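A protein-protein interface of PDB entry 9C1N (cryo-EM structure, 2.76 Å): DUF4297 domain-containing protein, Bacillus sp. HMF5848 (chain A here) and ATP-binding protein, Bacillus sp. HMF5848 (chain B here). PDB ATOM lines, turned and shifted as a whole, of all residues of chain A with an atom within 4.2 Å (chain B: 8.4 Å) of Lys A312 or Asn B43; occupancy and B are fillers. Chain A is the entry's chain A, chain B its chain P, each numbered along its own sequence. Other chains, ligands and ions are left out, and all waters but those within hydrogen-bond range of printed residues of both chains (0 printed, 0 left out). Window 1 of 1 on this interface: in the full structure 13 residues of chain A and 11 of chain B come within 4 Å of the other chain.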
ATOM      1  N   LEU A 275     -25.741  10.118  -3.970  1.00  0.00           N
ATOM      2  CA  LEU A 275     -24.957   8.893  -3.975  1.00  0.00           C
ATOM      3  C   LEU A 275     -23.469   9.172  -3.835  1.00  0.00           C
ATOM      4  O   LEU A 275     -22.674   8.229  -3.751  1.00  0.00           O
ATOM      5  CB  LEU A 275     -25.220   8.093  -5.257  1.00  0.00           C
ATOM      6  CG  LEU A 275     -26.345   7.058  -5.204  1.00  0.00           C
ATOM      7  CD1 LEU A 275     -26.393   6.253  -6.494  1.00  0.00           C
ATOM      8  CD2 LEU A 275     -26.176   6.140  -4.004  1.00  0.00           C
ATOM      9  N   ASN A 276     -23.080  10.445  -3.815  1.00  0.00           N
ATOM     10  CA  ASN A 276     -21.704  10.866  -3.609  1.00  0.00           C
ATOM     11  C   ASN A 276     -21.442  11.319  -2.177  1.00  0.00           C
ATOM     12  O   ASN A 276     -20.316  11.719  -1.861  1.00  0.00           O
ATOM     13  CB  ASN A 276     -21.354  11.993  -4.588  1.00  0.00           C
ATOM     14  CG  ASN A 276     -19.860  12.191  -4.746  1.00  0.00           C
ATOM     15  OD1 ASN A 276     -19.140  11.281  -5.159  1.00  0.00           O
ATOM     16  ND2 ASN A 276     -19.385  13.388  -4.423  1.00  0.00           N
ATOM     17  N   ILE A 277     -22.448  11.266  -1.310  1.00  0.00           N
ATOM     18  CA  ILE A 277     -22.307  11.680   0.081  1.00  0.00           C
ATOM     19  C   ILE A 277     -21.954  10.462   0.921  1.00  0.00           C
ATOM     20  O   ILE A 277     -22.618   9.421   0.833  1.00  0.00           O
ATOM     21  CB  ILE A 277     -23.594  12.352   0.590  1.00  0.00           C
ATOM     22  CG1 ILE A 277     -24.178  13.267  -0.487  1.00  0.00           C
ATOM     23  CG2 ILE A 277     -23.319  13.135   1.863  1.00  0.00           C
ATOM     24  CD1 ILE A 277     -25.489  13.914  -0.095  1.00  0.00           C
ATOM     25  N   ASN A 278     -20.901  10.585   1.732  1.00  0.00           N
ATOM     26  CA  ASN A 278     -20.431   9.454   2.525  1.00  0.00           C
ATOM     27  C   ASN A 278     -21.451   9.056   3.586  1.00  0.00           C
ATOM     28  O   ASN A 278     -21.816   7.880   3.701  1.00  0.00           O
ATOM     29  CB  ASN A 278     -19.089   9.792   3.173  1.00  0.00           C
ATOM     30  CG  ASN A 278     -18.002  10.070   2.152  1.00  0.00           C
ATOM     31  OD1 ASN A 278     -17.630   9.197   1.369  1.00  0.00           O
ATOM     32  ND2 ASN A 278     -17.486  11.293   2.159  1.00  0.00           N
ATOM     33  N   ARG A 282     -29.442   5.002   3.389  1.00  0.00           N
ATOM     34  CA  ARG A 282     -30.151   4.499   2.220  1.00  0.00           C
ATOM     35  C   ARG A 282     -30.839   3.191   2.586  1.00  0.00           C
ATOM     36  O   ARG A 282     -30.182   2.241   3.026  1.00  0.00           O
ATOM     37  CB  ARG A 282     -29.191   4.297   1.046  1.00  0.00           C
ATOM     38  CG  ARG A 282     -28.243   5.465   0.825  1.00  0.00           C
ATOM     39  CD  ARG A 282     -27.353   5.240  -0.387  1.00  0.00           C
ATOM     40  NE  ARG A 282     -26.531   6.405  -0.683  1.00  0.00           N
ATOM     41  CZ  ARG A 282     -25.353   6.653  -0.126  1.00  0.00           C
ATOM     42  NH1 ARG A 282     -24.824   5.831   0.766  1.00  0.00           N
ATOM     43  NH2 ARG A 282     -24.688   7.750  -0.472  1.00  0.00           N
ATOM     44  N   LYS A 308     -18.201  -0.217  -1.848  1.00  0.00           N
ATOM     45  CA  LYS A 308     -18.224   1.105  -2.464  1.00  0.00           C
ATOM     46  C   LYS A 308     -18.881   2.163  -1.594  1.00  0.00           C
ATOM     47  O   LYS A 308     -18.416   3.306  -1.567  1.00  0.00           O
ATOM     48  CB  LYS A 308     -18.944   1.051  -3.820  1.00  0.00           C
ATOM     49  CG  LYS A 308     -18.782   2.317  -4.646  1.00  0.00           C
ATOM     50  CD  LYS A 308     -19.237   2.115  -6.081  1.00  0.00           C
ATOM     51  CE  LYS A 308     -19.126   3.410  -6.867  1.00  0.00           C
ATOM     52  NZ  LYS A 308     -17.788   4.041  -6.707  1.00  0.00           N
ATOM     53  N   TYR A 309     -19.951   1.816  -0.875  1.00  0.00           N
ATOM     54  CA  TYR A 309     -20.683   2.778  -0.061  1.00  0.00           C
ATOM     55  C   TYR A 309     -20.560   2.536   1.438  1.00  0.00           C
ATOM     56  O   TYR A 309     -20.993   3.390   2.218  1.00  0.00           O
ATOM     57  CB  TYR A 309     -22.171   2.779  -0.443  1.00  0.00           C
ATOM     58  CG  TYR A 309     -22.443   3.186  -1.874  1.00  0.00           C
ATOM     59  CD1 TYR A 309     -22.524   4.524  -2.231  1.00  0.00           C
ATOM     60  CD2 TYR A 309     -22.629   2.234  -2.866  1.00  0.00           C
ATOM     61  CE1 TYR A 309     -22.774   4.902  -3.538  1.00  0.00           C
ATOM     62  CE2 TYR A 309     -22.880   2.602  -4.174  1.00  0.00           C
ATOM     63  CZ  TYR A 309     -22.951   3.938  -4.505  1.00  0.00           C
ATOM     64  OH  TYR A 309     -23.202   4.313  -5.805  1.00  0.00           O
ATOM     65  N   ASN A 310     -19.995   1.407   1.861  1.00  0.00           N
ATOM     66  CA  ASN A 310     -19.872   1.087   3.279  1.00  0.00           C
ATOM     67  C   ASN A 310     -18.491   0.520   3.576  1.00  0.00           C
ATOM     68  O   ASN A 310     -18.348  -0.473   4.297  1.00  0.00           O
ATOM     69  CB  ASN A 310     -20.964   0.115   3.723  1.00  0.00           C
ATOM     70  CG  ASN A 310     -21.210   0.158   5.217  1.00  0.00           C
ATOM     71  OD1 ASN A 310     -20.594   0.947   5.937  1.00  0.00           O
ATOM     72  ND2 ASN A 310     -22.109  -0.695   5.694  1.00  0.00           N
ATOM     73  N   SER A 311     -17.452   1.139   3.017  1.00  0.00           N
ATOM     74  CA  SER A 311     -16.084   0.661   3.174  1.00  0.00           C
ATOM     75  C   SER A 311     -15.267   1.488   4.156  1.00  0.00           C
ATOM     76  O   SER A 311     -14.531   0.922   4.971  1.00  0.00           O
ATOM     77  CB  SER A 311     -15.374   0.640   1.815  1.00  0.00           C
ATOM     78  OG  SER A 311     -15.209   1.949   1.305  1.00  0.00           O
ATOM     79  N   LYS A 312     -15.369   2.813   4.097  1.00  0.00           N
ATOM     80  CA  LYS A 312     -14.617   3.661   5.010  1.00  0.00           C
ATOM     81  C   LYS A 312     -15.141   3.511   6.433  1.00  0.00           C
ATOM     82  O   LYS A 312     -16.350   3.511   6.673  1.00  0.00           O
ATOM     83  CB  LYS A 312     -14.694   5.120   4.563  1.00  0.00           C
ATOM     84  CG  LYS A 312     -14.106   5.368   3.183  1.00  0.00           C
ATOM     85  CD  LYS A 312     -14.921   6.391   2.409  1.00  0.00           C
ATOM     86  CE  LYS A 312     -14.526   6.408   0.941  1.00  0.00           C
ATOM     87  NZ  LYS A 312     -15.181   7.525   0.204  1.00  0.00           N
ATOM     88  N   ILE A 313     -14.212   3.390   7.383  1.00  0.00           N
ATOM     89  CA  ILE A 313     -14.579   3.129   8.770  1.00  0.00           C
ATOM     90  C   ILE A 313     -14.904   4.408   9.539  1.00  0.00           C
ATOM     91  O   ILE A 313     -15.550   4.338  10.597  1.00  0.00           O
ATOM     92  CB  ILE A 313     -13.458   2.341   9.471  1.00  0.00           C
ATOM     93  CG1 ILE A 313     -13.930   1.781  10.816  1.00  0.00           C
ATOM     94  CG2 ILE A 313     -12.222   3.211   9.652  1.00  0.00           C
ATOM     95  CD1 ILE A 313     -15.015   0.732  10.692  1.00  0.00           C
ATOM     96  N   LYS A 314     -14.495   5.572   9.038  1.00  0.00           N
ATOM     97  CA  LYS A 314     -14.734   6.836   9.719  1.00  0.00           C
ATOM     98  C   LYS A 314     -15.717   7.746   8.996  1.00  0.00           C
ATOM     99  O   LYS A 314     -16.388   8.550   9.647  1.00  0.00           O
ATOM    100  CB  LYS A 314     -13.409   7.587   9.920  1.00  0.00           C
ATOM    101  CG  LYS A 314     -13.528   8.903  10.678  1.00  0.00           C
ATOM    102  CD  LYS A 314     -12.164   9.525  10.930  1.00  0.00           C
ATOM    103  CE  LYS A 314     -12.295  10.906  11.552  1.00  0.00           C
ATOM    104  NZ  LYS A 314     -12.882  10.844  12.918  1.00  0.00           N
ATOM    105  N   LEU A 315     -15.832   7.629   7.674  1.00  0.00           N
ATOM    106  CA  LEU A 315     -16.709   8.486   6.885  1.00  0.00           C
ATOM    107  C   LEU A 315     -18.044   7.830   6.552  1.00  0.00           C
ATOM    108  O   LEU A 315     -19.076   8.508   6.547  1.00  0.00           O
ATOM    109  CB  LEU A 315     -16.006   8.898   5.588  1.00  0.00           C
ATOM    110  CG  LEU A 315     -14.703   9.679   5.781  1.00  0.00           C
ATOM    111  CD1 LEU A 315     -13.827   9.555   4.554  1.00  0.00           C
ATOM    112  CD2 LEU A 315     -14.985  11.138   6.084  1.00  0.00           C
ATOM    113  N   HIS A 316     -18.051   6.528   6.272  1.00  0.00           N
ATOM    114  CA  HIS A 316     -19.281   5.793   5.978  1.00  0.00           C
ATOM    115  C   HIS A 316     -19.842   5.296   7.305  1.00  0.00           C
ATOM    116  O   HIS A 316     -19.559   4.182   7.748  1.00  0.00           O
ATOM    117  CB  HIS A 316     -19.006   4.649   5.010  1.00  0.00           C
ATOM    118  CG  HIS A 316     -18.797   5.092   3.594  1.00  0.00           C
ATOM    119  ND1 HIS A 316     -18.073   4.353   2.683  1.00  0.00           N
ATOM    120  CD2 HIS A 316     -19.209   6.200   2.935  1.00  0.00           C
ATOM    121  CE1 HIS A 316     -18.052   4.985   1.525  1.00  0.00           C
ATOM    122  NE2 HIS A 316     -18.734   6.108   1.651  1.00  0.00           N
ATOM    123  N   MET B   1      -8.001   2.306   0.842  1.00  0.00           N
ATOM    124  CA  MET B   1      -6.677   2.917   0.855  1.00  0.00           C
ATOM    125  C   MET B   1      -5.697   2.115   0.004  1.00  0.00           C
ATOM    126  O   MET B   1      -5.615   0.893   0.118  1.00  0.00           O
ATOM    127  CB  MET B   1      -6.153   3.032   2.287  1.00  0.00           C
ATOM    128  CG  MET B   1      -6.772   4.166   3.089  1.00  0.00           C
ATOM    129  SD  MET B   1      -8.474   3.821   3.573  1.00  0.00           S
ATOM    130  CE  MET B   1      -8.217   2.618   4.874  1.00  0.00           C
ATOM    131  N   GLN B  40      -9.617  10.855  -3.057  1.00  0.00           N
ATOM    132  CA  GLN B  40     -11.049  10.678  -3.228  1.00  0.00           C
ATOM    133  C   GLN B  40     -11.818  11.786  -2.517  1.00  0.00           C
ATOM    134  O   GLN B  40     -11.423  12.250  -1.443  1.00  0.00           O
ATOM    135  CB  GLN B  40     -11.478   9.310  -2.699  1.00  0.00           C
ATOM    136  CG  GLN B  40     -12.791   8.808  -3.268  1.00  0.00           C
ATOM    137  CD  GLN B  40     -13.002   7.328  -3.018  1.00  0.00           C
ATOM    138  OE1 GLN B  40     -12.101   6.631  -2.548  1.00  0.00           O
ATOM    139  NE2 GLN B  40     -14.196   6.838  -3.331  1.00  0.00           N
ATOM    140  N   GLU B  41     -12.917  12.214  -3.131  1.00  0.00           N
ATOM    141  CA  GLU B  41     -13.830  13.194  -2.550  1.00  0.00           C
ATOM    142  C   GLU B  41     -15.240  12.662  -2.776  1.00  0.00           C
ATOM    143  O   GLU B  41     -15.787  12.780  -3.875  1.00  0.00           O
ATOM    144  CB  GLU B  41     -13.639  14.574  -3.175  1.00  0.00           C
ATOM    145  CG  GLU B  41     -14.210  15.723  -2.353  1.00  0.00           C
ATOM    146  CD  GLU B  41     -15.727  15.764  -2.366  1.00  0.00           C
ATOM    147  OE1 GLU B  41     -16.315  15.706  -3.466  1.00  0.00           O
ATOM    148  OE2 GLU B  41     -16.330  15.847  -1.277  1.00  0.00           O
ATOM    149  N   GLY B  42     -15.828  12.073  -1.741  1.00  0.00           N
ATOM    150  CA  GLY B  42     -17.103  11.415  -1.895  1.00  0.00           C
ATOM    151  C   GLY B  42     -16.948  10.037  -2.512  1.00  0.00           C
ATOM    152  O   GLY B  42     -15.841   9.528  -2.721  1.00  0.00           O
ATOM    153  N   ASN B  43     -18.093   9.426  -2.813  1.00  0.00           N
ATOM    154  CA  ASN B  43     -18.101   8.062  -3.328  1.00  0.00           C
ATOM    155  C   ASN B  43     -17.717   7.971  -4.799  1.00  0.00           C
ATOM    156  O   ASN B  43     -17.294   6.898  -5.245  1.00  0.00           O
ATOM    157  CB  ASN B  43     -19.480   7.432  -3.123  1.00  0.00           C
ATOM    158  CG  ASN B  43     -19.875   7.358  -1.660  1.00  0.00           C
ATOM    159  OD1 ASN B  43     -19.018   7.293  -0.777  1.00  0.00           O
ATOM    160  ND2 ASN B  43     -21.177   7.370  -1.398  1.00  0.00           N
ATOM    161  N   HIS B  44     -17.845   9.058  -5.562  1.00  0.00           N
ATOM    162  CA  HIS B  44     -17.666   8.999  -7.007  1.00  0.00           C
ATOM    163  C   HIS B  44     -16.651   9.987  -7.564  1.00  0.00           C
ATOM    164  O   HIS B  44     -16.256   9.837  -8.725  1.00  0.00           O
ATOM    165  CB  HIS B  44     -19.009   9.230  -7.718  1.00  0.00           C
ATOM    166  CG  HIS B  44     -20.014   8.148  -7.478  1.00  0.00           C
ATOM    167  ND1 HIS B  44     -21.359   8.405  -7.327  1.00  0.00           N
ATOM    168  CD2 HIS B  44     -19.871   6.808  -7.358  1.00  0.00           C
ATOM    169  CE1 HIS B  44     -22.002   7.269  -7.126  1.00  0.00           C
ATOM    170  NE2 HIS B  44     -21.122   6.285  -7.140  1.00  0.00           N
ATOM    171  N   ASN B  45     -16.218  10.979  -6.793  1.00  0.00           N
ATOM    172  CA  ASN B  45     -15.375  12.049  -7.300  1.00  0.00           C
ATOM    173  C   ASN B  45     -13.948  11.897  -6.790  1.00  0.00           C
ATOM    174  O   ASN B  45     -13.710  11.367  -5.701  1.00  0.00           O
ATOM    175  CB  ASN B  45     -15.933  13.417  -6.896  1.00  0.00           C
ATOM    176  CG  ASN B  45     -17.269  13.714  -7.545  1.00  0.00           C
ATOM    177  OD1 ASN B  45     -17.754  12.947  -8.378  1.00  0.00           O
ATOM    178  ND2 ASN B  45     -17.885  14.820  -7.147  1.00  0.00           N
ATOM    179  N   PHE B  46     -12.997  12.373  -7.593  1.00  0.00           N
ATOM    180  CA  PHE B  46     -11.583  12.325  -7.258  1.00  0.00           C
ATOM    181  C   PHE B  46     -10.984  13.717  -7.381  1.00  0.00           C
ATOM    182  O   PHE B  46     -11.421  14.529  -8.202  1.00  0.00           O
ATOM    183  CB  PHE B  46     -10.816  11.356  -8.168  1.00  0.00           C
ATOM    184  CG  PHE B  46     -11.116   9.908  -7.906  1.00  0.00           C
ATOM    185  CD1 PHE B  46     -10.410   9.202  -6.951  1.00  0.00           C
ATOM    186  CD2 PHE B  46     -12.103   9.253  -8.623  1.00  0.00           C
ATOM    187  CE1 PHE B  46     -10.684   7.870  -6.711  1.00  0.00           C
ATOM    188  CE2 PHE B  46     -12.381   7.922  -8.387  1.00  0.00           C
ATOM    189  CZ  PHE B  46     -11.670   7.230  -7.430  1.00  0.00           C
ATOM    190  N   PHE B  75     -12.424  15.383 -10.539  1.00  0.00           N
ATOM    191  CA  PHE B  75     -12.929  14.408 -11.503  1.00  0.00           C
ATOM    192  C   PHE B  75     -14.395  14.131 -11.183  1.00  0.00           C
ATOM    193  O   PHE B  75     -14.713  13.255 -10.374  1.00  0.00           O
ATOM    194  CB  PHE B  75     -12.098  13.125 -11.476  1.00  0.00           C
ATOM    195  CG  PHE B  75     -11.041  13.067 -12.539  1.00  0.00           C
ATOM    196  CD1 PHE B  75     -11.325  12.539 -13.787  1.00  0.00           C
ATOM    197  CD2 PHE B  75      -9.764  13.541 -12.290  1.00  0.00           C
ATOM    198  CE1 PHE B  75     -10.354  12.486 -14.767  1.00  0.00           C
ATOM    199  CE2 PHE B  75      -8.791  13.489 -13.267  1.00  0.00           C
ATOM    200  CZ  PHE B  75      -9.088  12.961 -14.505  1.00  0.00           C
ATOM    201  N   SER B  89     -12.381  15.313   2.777  1.00  0.00           N
ATOM    202  CA  SER B  89     -12.536  15.043   4.197  1.00  0.00           C
ATOM    203  C   SER B  89     -11.385  14.173   4.708  1.00  0.00           C
ATOM    204  O   SER B  89     -10.792  13.409   3.945  1.00  0.00           O
ATOM    205  CB  SER B  89     -13.868  14.345   4.460  1.00  0.00           C
ATOM    206  OG  SER B  89     -14.235  14.422   5.826  1.00  0.00           O
ATOM    207  N   PRO B  90     -11.052  14.274   5.997  1.00  0.00           N
ATOM    208  CA  PRO B  90      -9.966  13.453   6.548  1.00  0.00           C
ATOM    209  C   PRO B  90     -10.252  11.964   6.422  1.00  0.00           C
ATOM    210  O   PRO B  90     -11.396  11.527   6.279  1.00  0.00           O
ATOM    211  CB  PRO B  90      -9.909  13.884   8.016  1.00  0.00           C
ATOM    212  CG  PRO B  90     -10.388  15.285   7.998  1.00  0.00           C
ATOM    213  CD  PRO B  90     -11.458  15.338   6.933  1.00  0.00           C
ATOM    214  N   THR B  91      -9.173  11.179   6.489  1.00  0.00           N
ATOM    215  CA  THR B  91      -9.218   9.723   6.322  1.00  0.00           C
ATOM    216  C   THR B  91      -9.874   9.332   4.997  1.00  0.00           C
ATOM    217  O   THR B  91     -10.705   8.424   4.937  1.00  0.00           O
ATOM    218  CB  THR B  91      -9.917   9.037   7.502  1.00  0.00           C
ATOM    219  OG1 THR B  91     -11.276   9.485   7.600  1.00  0.00           O
ATOM    220  CG2 THR B  91      -9.189   9.347   8.805  1.00  0.00           C
ATOM    221  N   GLU B  92      -9.493  10.029   3.925  1.00  0.00           N
ATOM    222  CA  GLU B  92      -9.898   9.695   2.569  1.00  0.00           C
ATOM    223  C   GLU B  92      -8.728   9.066   1.832  1.00  0.00           C
ATOM    224  O   GLU B  92      -7.602   9.574   1.917  1.00  0.00           O
ATOM    225  CB  GLU B  92     -10.382  10.943   1.820  1.00  0.00           C
ATOM    226  CG  GLU B  92     -11.876  11.210   1.951  1.00  0.00           C
ATOM    227  CD  GLU B  92     -12.717  10.256   1.124  1.00  0.00           C
ATOM    228  OE1 GLU B  92     -12.939   9.113   1.570  1.00  0.00           O
ATOM    229  OE2 GLU B  92     -13.169  10.652   0.030  1.00  0.00           O
ATOM    230  N   PRO B  93      -8.948   7.965   1.116  1.00  0.00           N
ATOM    231  CA  PRO B  93      -7.825   7.250   0.496  1.00  0.00           C
ATOM    232  C   PRO B  93      -7.144   8.057  -0.602  1.00  0.00           C
ATOM    233  O   PRO B  93      -7.751   8.910  -1.254  1.00  0.00           O
ATOM    234  CB  PRO B  93      -8.480   5.986  -0.078  1.00  0.00           C
ATOM    235  CG  PRO B  93      -9.946   6.274  -0.105  1.00  0.00           C
ATOM    236  CD  PRO B  93     -10.213   7.221   1.012  1.00  0.00           C
ATOM    237  N   PHE B  95      -4.885   7.314  -4.101  1.00  0.00           N
ATOM    238  CA  PHE B  95      -4.992   6.159  -4.988  1.00  0.00           C
ATOM    239  C   PHE B  95      -3.971   6.112  -6.122  1.00  0.00           C
ATOM    240  O   PHE B  95      -4.126   5.283  -7.027  1.00  0.00           O
ATOM    241  CB  PHE B  95      -6.407   6.084  -5.567  1.00  0.00           C
ATOM    242  CG  PHE B  95      -7.307   5.132  -4.832  1.00  0.00           C
ATOM    243  CD1 PHE B  95      -7.125   3.763  -4.938  1.00  0.00           C
ATOM    244  CD2 PHE B  95      -8.328   5.605  -4.025  1.00  0.00           C
ATOM    245  CE1 PHE B  95      -7.948   2.886  -4.259  1.00  0.00           C
ATOM    246  CE2 PHE B  95      -9.154   4.732  -3.344  1.00  0.00           C
ATOM    247  CZ  PHE B  95      -8.963   3.372  -3.462  1.00  0.00           C
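The backbone carbonyl oxygen of Ile A277 is in hydrogen-bond range of the guanidinium group of Arg A282 (3.0 Å).
The side-chain amide oxygen (OD1) of Asn A278 is in hydrogen-bond range of a ring nitrogen (NE2) of His A316 (3.3 Å).
N of Lys A312 lies within hydrogen-bond range of ND1 of His A316, at 3.4 Å.
O of Gly B42 sits close to NE2 of Gln B40 (3.2 Å).
N of Gln B40 lies within hydrogen-bond range of O of Pro B93 (3.2 Å).
N of Gly B42 is in hydrogen-bond range of OE2 of Glu B92 (3.5 Å).
Of the 15 printed residues of chain B, 10 touch a printed residue of chain A.
Along chain B the printed residues that touch a printed residue of chain A span positions 40 to 92.
Among the printed residues, Asp or Glu carboxylates within 4 Å of a Lys or Arg side-chain nitrogen of the other chain: Lys A312 with Glu B92 (3.1 Å).
Among the printed residues, merely in contact across the chains: Leu A315 with Glu B92, Asn A276 with Gly B42, Tyr A309 with Asn B43, Leu A315 with Thr B91, Leu A315 with Ser B89, Lys A314 with Thr B91, Lys A308 with His B44, Leu A275 with His B44, Leu A315 with Pro B90, Lys A312 with Gly B42, Arg A282 with Asn B43, Asn A276 with Glu B41, Lys A312 with Gln B40, Lys A312 with Asn B43 and Asn A278 with Gly B42.
ND2 of Asn B43 is in hydrogen-bond range of O of Leu A275 (2.9 Å).
The backbone NH (N) of Asn B43 sits at hydrogen-bond distance from the side-chain amide oxygen (OD1) of Asn A276 (3.2 Å).
N of His B44 sits at hydrogen-bond distance from OD1 of Asn A276, at 2.6 Å.
The side-chain amide oxygen of Asn A276 sits at hydrogen-bond distance from the backbone NH of Asn B45 (3.4 Å).
The backbone carbonyl oxygen (O) of Ile A277 sits at hydrogen-bond distance from the side-chain amide nitrogen (ND2) of Asn B43.
OD1 of Asn B43 lies close to OD1 of Asn A278, 3.2 Å away.
The backbone carbonyl oxygen (O) of Asn B43 lies within hydrogen-bond range of the side-chain amino group (NZ) of Lys A308 (3.2 Å).
A ring nitrogen (NE2) of His B44 sits at hydrogen-bond distance from the side-chain hydroxyl (OH) of Tyr A309 (3.2 Å).
NZ of Lys A312 is in salt-bridge range of OE1 of Glu B92 (3.1 Å).
NE2 of His A316 lies within hydrogen-bond range of OD1 of Asn B43, 2.7 Å away.
Of the printed residues of chain B, Leu A275 touches Asn B43 and His B44.
No residue of chain B comes within 4 Å of Ser A311.
Lys A312 touches four residues of chain B.
Printed residues of chain B within 4 Å of Lys A314: Thr B91.
Printed residues of chain A within 4 Å of Glu B41: Asn A276.
Printed residues of chain A within 4 Å of Gly B42: Asn A276, Asn A278 and Lys A312.
Of chain A, only Leu A275, Asn A276, Ile A277, Asn A278, Arg A282, Lys A308, Tyr A309, Lys A312 and His A316 come within 4 Å of Asn B43.
Of the printed residues of chain A, Ser B89 touches Leu A315 (3.4 Å).
The nearest printed residue of chain A that does not touch Asn B43 is Asn A310 (6.5 Å).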
